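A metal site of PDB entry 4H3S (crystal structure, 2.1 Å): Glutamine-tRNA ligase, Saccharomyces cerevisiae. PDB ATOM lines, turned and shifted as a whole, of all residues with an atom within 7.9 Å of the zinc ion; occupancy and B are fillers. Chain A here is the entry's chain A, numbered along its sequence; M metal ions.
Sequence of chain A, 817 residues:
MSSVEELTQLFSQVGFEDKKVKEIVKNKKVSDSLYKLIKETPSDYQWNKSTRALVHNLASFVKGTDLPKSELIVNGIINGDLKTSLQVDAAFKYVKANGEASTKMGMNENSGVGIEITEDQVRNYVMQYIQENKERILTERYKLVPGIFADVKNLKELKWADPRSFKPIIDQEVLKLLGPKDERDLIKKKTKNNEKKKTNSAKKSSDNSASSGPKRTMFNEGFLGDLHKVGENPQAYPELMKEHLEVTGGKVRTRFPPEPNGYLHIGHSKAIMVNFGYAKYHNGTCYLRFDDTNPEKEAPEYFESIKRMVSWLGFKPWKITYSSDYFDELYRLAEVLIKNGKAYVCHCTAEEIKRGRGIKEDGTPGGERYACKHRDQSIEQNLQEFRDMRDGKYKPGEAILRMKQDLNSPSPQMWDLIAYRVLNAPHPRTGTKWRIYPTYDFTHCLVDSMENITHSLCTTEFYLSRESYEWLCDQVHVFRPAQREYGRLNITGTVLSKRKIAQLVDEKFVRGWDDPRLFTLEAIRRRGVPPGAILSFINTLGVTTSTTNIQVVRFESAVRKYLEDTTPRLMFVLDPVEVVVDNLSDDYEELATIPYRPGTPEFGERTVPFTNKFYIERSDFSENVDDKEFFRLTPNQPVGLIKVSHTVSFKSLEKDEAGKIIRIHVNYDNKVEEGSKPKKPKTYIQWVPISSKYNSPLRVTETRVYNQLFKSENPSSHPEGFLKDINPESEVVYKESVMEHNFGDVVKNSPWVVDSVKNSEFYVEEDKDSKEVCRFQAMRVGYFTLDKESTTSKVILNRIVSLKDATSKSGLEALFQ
His 347 touches the zinc ion. Five residues have an atom within 4 Å of the zinc ion: Cys 346, His 347, Cys 348, Cys 372 and His 374. The nearest printed residue that does not touch the zinc ion is Arg 402 (4.6 Å).
A ring nitrogen (ND1) of His 374 sits close to the backbone NH of His 347, at 3.4 Å. SG of Cys 346 sits close to NH1 of Arg 402. The backbone NH (N) of Cys 346 lies within hydrogen-bond range of the backbone carbonyl oxygen (O) of Ile 400 (2.8 Å).
The zinc ion is bound by ND1 of His 374 (2.0 Å), SG of Cys 346 (2.3 Å), SG of Cys 372 (2.3 Å) and SG of Cys 348 (2.4 Å). The zinc ion has four donor atoms within binding distance.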
ATOM      1  N   TYR A 344      -2.834  21.264 -17.665  1.00  0.00           N
ATOM      2  CA  TYR A 344      -2.316  21.784 -18.926  1.00  0.00           C
ATOM      3  C   TYR A 344      -3.405  21.832 -19.984  1.00  0.00           C
ATOM      4  O   TYR A 344      -4.395  21.107 -19.905  1.00  0.00           O
ATOM      5  CB  TYR A 344      -1.132  20.932 -19.413  1.00  0.00           C
ATOM      6  CG  TYR A 344      -1.447  19.475 -19.668  1.00  0.00           C
ATOM      7  CD1 TYR A 344      -1.569  18.575 -18.625  1.00  0.00           C
ATOM      8  CD2 TYR A 344      -1.588  18.995 -20.964  1.00  0.00           C
ATOM      9  CE1 TYR A 344      -1.843  17.242 -18.851  1.00  0.00           C
ATOM     10  CE2 TYR A 344      -1.866  17.663 -21.209  1.00  0.00           C
ATOM     11  CZ  TYR A 344      -1.987  16.791 -20.144  1.00  0.00           C
ATOM     12  OH  TYR A 344      -2.263  15.458 -20.379  1.00  0.00           O
ATOM     13  N   VAL A 345      -3.216  22.704 -20.972  1.00  0.00           N
ATOM     14  CA  VAL A 345      -4.155  22.783 -22.082  1.00  0.00           C
ATOM     15  C   VAL A 345      -3.693  21.858 -23.193  1.00  0.00           C
ATOM     16  O   VAL A 345      -2.603  22.021 -23.733  1.00  0.00           O
ATOM     17  CB  VAL A 345      -4.292  24.212 -22.610  1.00  0.00           C
ATOM     18  CG1 VAL A 345      -5.144  24.235 -23.877  1.00  0.00           C
ATOM     19  CG2 VAL A 345      -4.895  25.115 -21.541  1.00  0.00           C
ATOM     20  N   CYS A 346      -4.529  20.885 -23.515  1.00  0.00           N
ATOM     21  CA  CYS A 346      -4.210  19.860 -24.489  1.00  0.00           C
ATOM     22  C   CYS A 346      -5.026  20.079 -25.760  1.00  0.00           C
ATOM     23  O   CYS A 346      -6.176  20.530 -25.699  1.00  0.00           O
ATOM     24  CB  CYS A 346      -4.518  18.485 -23.888  1.00  0.00           C
ATOM     25  SG  CYS A 346      -4.333  17.084 -25.002  1.00  0.00           S
ATOM     26  N   HIS A 347      -4.438  19.778 -26.908  1.00  0.00           N
ATOM     27  CA  HIS A 347      -5.115  19.934 -28.194  1.00  0.00           C
ATOM     28  C   HIS A 347      -5.180  18.602 -28.939  1.00  0.00           C
ATOM     29  O   HIS A 347      -5.327  18.580 -30.171  1.00  0.00           O
ATOM     30  CB  HIS A 347      -4.396  20.975 -29.053  1.00  0.00           C
ATOM     31  CG  HIS A 347      -4.204  22.286 -28.359  1.00  0.00           C
ATOM     32  ND1 HIS A 347      -5.205  23.235 -28.255  1.00  0.00           N
ATOM     33  CD2 HIS A 347      -3.125  22.811 -27.711  1.00  0.00           C
ATOM     34  CE1 HIS A 347      -4.750  24.285 -27.596  1.00  0.00           C
ATOM     35  NE2 HIS A 347      -3.491  24.051 -27.257  1.00  0.00           N
ATOM     36  N   CYS A 348      -5.074  17.504 -28.206  1.00  0.00           N
ATOM     37  CA  CYS A 348      -5.150  16.177 -28.805  1.00  0.00           C
ATOM     38  C   CYS A 348      -6.592  15.816 -29.165  1.00  0.00           C
ATOM     39  O   CYS A 348      -7.525  16.202 -28.468  1.00  0.00           O
ATOM     40  CB  CYS A 348      -4.580  15.121 -27.854  1.00  0.00           C
ATOM     41  SG  CYS A 348      -2.795  15.174 -27.674  1.00  0.00           S
ATOM     42  N   THR A 349      -6.756  15.071 -30.248  1.00  0.00           N
ATOM     43  CA  THR A 349      -8.059  14.566 -30.629  1.00  0.00           C
ATOM     44  C   THR A 349      -8.469  13.449 -29.669  1.00  0.00           C
ATOM     45  O   THR A 349      -7.651  12.954 -28.900  1.00  0.00           O
ATOM     46  CB  THR A 349      -8.046  14.015 -32.066  1.00  0.00           C
ATOM     47  OG1 THR A 349      -7.138  12.900 -32.129  1.00  0.00           O
ATOM     48  CG2 THR A 349      -7.602  15.077 -33.047  1.00  0.00           C
ATOM     49  N   GLU A 352      -6.276  10.488 -30.270  1.00  0.00           N
ATOM     50  CA  GLU A 352      -4.911  10.687 -29.790  1.00  0.00           C
ATOM     51  C   GLU A 352      -4.846  10.561 -28.263  1.00  0.00           C
ATOM     52  O   GLU A 352      -3.862  10.085 -27.714  1.00  0.00           O
ATOM     53  CB  GLU A 352      -4.393  12.051 -30.233  1.00  0.00           C
ATOM     54  CG  GLU A 352      -4.103  12.132 -31.719  1.00  0.00           C
ATOM     55  CD  GLU A 352      -3.814  13.553 -32.189  1.00  0.00           C
ATOM     56  OE1 GLU A 352      -4.190  14.505 -31.475  1.00  0.00           O
ATOM     57  OE2 GLU A 352      -3.200  13.713 -33.270  1.00  0.00           O
ATOM     58  N   ILE A 353      -5.915  10.985 -27.595  1.00  0.00           N
ATOM     59  CA  ILE A 353      -6.001  10.859 -26.147  1.00  0.00           C
ATOM     60  C   ILE A 353      -6.103   9.386 -25.753  1.00  0.00           C
ATOM     61  O   ILE A 353      -5.431   8.930 -24.825  1.00  0.00           O
ATOM     62  CB  ILE A 353      -7.179  11.653 -25.573  1.00  0.00           C
ATOM     63  CG1 ILE A 353      -6.889  13.158 -25.647  1.00  0.00           C
ATOM     64  CG2 ILE A 353      -7.467  11.253 -24.129  1.00  0.00           C
ATOM     65  CD1 ILE A 353      -8.081  14.049 -25.361  1.00  0.00           C
ATOM     66  N   ALA A 371       2.840  10.547 -22.563  1.00  0.00           N
ATOM     67  CA  ALA A 371       2.347  11.908 -22.576  1.00  0.00           C
ATOM     68  C   ALA A 371       2.412  12.521 -23.965  1.00  0.00           C
ATOM     69  O   ALA A 371       3.256  12.147 -24.785  1.00  0.00           O
ATOM     70  CB  ALA A 371       3.153  12.757 -21.608  1.00  0.00           C
ATOM     71  N   CYS A 372       1.507  13.456 -24.243  1.00  0.00           N
ATOM     72  CA  CYS A 372       1.576  14.244 -25.457  1.00  0.00           C
ATOM     73  C   CYS A 372       2.525  15.419 -25.208  1.00  0.00           C
ATOM     74  O   CYS A 372       2.965  15.636 -24.079  1.00  0.00           O
ATOM     75  CB  CYS A 372       0.186  14.762 -25.851  1.00  0.00           C
ATOM     76  SG  CYS A 372      -0.548  15.879 -24.635  1.00  0.00           S
ATOM     77  N   LYS A 373       2.818  16.188 -26.257  1.00  0.00           N
ATOM     78  CA  LYS A 373       3.716  17.327 -26.123  1.00  0.00           C
ATOM     79  C   LYS A 373       3.098  18.452 -25.281  1.00  0.00           C
ATOM     80  O   LYS A 373       3.820  19.279 -24.718  1.00  0.00           O
ATOM     81  CB  LYS A 373       4.115  17.855 -27.500  1.00  0.00           C
ATOM     82  CG  LYS A 373       4.938  16.862 -28.316  1.00  0.00           C
ATOM     83  CD  LYS A 373       6.113  17.544 -29.004  1.00  0.00           C
ATOM     84  CE  LYS A 373       7.040  16.525 -29.640  1.00  0.00           C
ATOM     85  NZ  LYS A 373       7.723  15.667 -28.619  1.00  0.00           N
ATOM     86  N   HIS A 374       1.781  18.478 -25.201  1.00  0.00           N
ATOM     87  CA  HIS A 374       1.090  19.547 -24.491  1.00  0.00           C
ATOM     88  C   HIS A 374       1.330  19.482 -22.978  1.00  0.00           C
ATOM     89  O   HIS A 374       1.271  20.492 -22.289  1.00  0.00           O
ATOM     90  CB  HIS A 374      -0.409  19.506 -24.776  1.00  0.00           C
ATOM     91  CG  HIS A 374      -0.737  19.384 -26.241  1.00  0.00           C
ATOM     92  ND1 HIS A 374      -1.374  18.281 -26.770  1.00  0.00           N
ATOM     93  CD2 HIS A 374      -0.501  20.215 -27.273  1.00  0.00           C
ATOM     94  CE1 HIS A 374      -1.520  18.447 -28.071  1.00  0.00           C
ATOM     95  NE2 HIS A 374      -1.003  19.608 -28.405  1.00  0.00           N
ATOM     96  N   ARG A 375       1.615  18.275 -22.488  1.00  0.00           N
ATOM     97  CA  ARG A 375       1.775  18.048 -21.060  1.00  0.00           C
ATOM     98  C   ARG A 375       2.967  18.813 -20.462  1.00  0.00           C
ATOM     99  O   ARG A 375       2.967  19.148 -19.289  1.00  0.00           O
ATOM    100  CB  ARG A 375       1.928  16.554 -20.787  1.00  0.00           C
ATOM    101  CG  ARG A 375       1.672  16.157 -19.340  1.00  0.00           C
ATOM    102  CD  ARG A 375       1.779  14.645 -19.149  1.00  0.00           C
ATOM    103  NE  ARG A 375       1.074  14.210 -17.944  1.00  0.00           N
ATOM    104  CZ  ARG A 375       1.585  14.203 -16.713  1.00  0.00           C
ATOM    105  NH1 ARG A 375       2.824  14.615 -16.499  1.00  0.00           N
ATOM    106  NH2 ARG A 375       0.835  13.791 -15.701  1.00  0.00           N
ATOM    107  N   GLN A 377       3.972  21.794 -21.292  1.00  0.00           N
ATOM    108  CA  GLN A 377       3.817  23.237 -21.456  1.00  0.00           C
ATOM    109  C   GLN A 377       4.014  24.016 -20.153  1.00  0.00           C
ATOM    110  O   GLN A 377       3.635  23.559 -19.073  1.00  0.00           O
ATOM    111  CB  GLN A 377       2.457  23.557 -22.076  1.00  0.00           C
ATOM    112  CG  GLN A 377       2.412  23.268 -23.574  1.00  0.00           C
ATOM    113  CD  GLN A 377       1.005  23.234 -24.146  1.00  0.00           C
ATOM    114  OE1 GLN A 377       0.828  22.910 -25.320  1.00  0.00           O
ATOM    115  NE2 GLN A 377       0.006  23.582 -23.345  1.00  0.00           N
ATOM    116  N   ILE A 400      -8.774  21.405 -24.669  1.00  0.00           N
ATOM    117  CA  ILE A 400      -9.309  20.972 -23.388  1.00  0.00           C
ATOM    118  C   ILE A 400      -8.289  21.257 -22.302  1.00  0.00           C
ATOM    119  O   ILE A 400      -7.090  21.285 -22.558  1.00  0.00           O
ATOM    120  CB  ILE A 400      -9.605  19.464 -23.395  1.00  0.00           C
ATOM    121  CG1 ILE A 400      -8.422  18.701 -23.979  1.00  0.00           C
ATOM    122  CG2 ILE A 400     -10.870  19.164 -24.192  1.00  0.00           C
ATOM    123  CD1 ILE A 400      -8.461  17.209 -23.734  1.00  0.00           C
ATOM    124  N   ARG A 402      -6.671  19.625 -19.120  1.00  0.00           N
ATOM    125  CA  ARG A 402      -6.530  18.319 -18.502  1.00  0.00           C
ATOM    126  C   ARG A 402      -5.769  18.433 -17.185  1.00  0.00           C
ATOM    127  O   ARG A 402      -4.856  19.240 -17.045  1.00  0.00           O
ATOM    128  CB  ARG A 402      -5.776  17.368 -19.423  1.00  0.00           C
ATOM    129  CG  ARG A 402      -6.453  17.135 -20.757  1.00  0.00           C
ATOM    130  CD  ARG A 402      -5.651  16.196 -21.637  1.00  0.00           C
ATOM    131  NE  ARG A 402      -5.638  14.835 -21.117  1.00  0.00           N
ATOM    132  CZ  ARG A 402      -5.100  13.802 -21.750  1.00  0.00           C
ATOM    133  NH1 ARG A 402      -4.520  13.969 -22.936  1.00  0.00           N
ATOM    134  NH2 ARG A 402      -5.134  12.596 -21.209  1.00  0.00           N
HETATM  135 ZN    ZN M   1      -2.301  16.701 -25.912  1.00  0.00          ZN
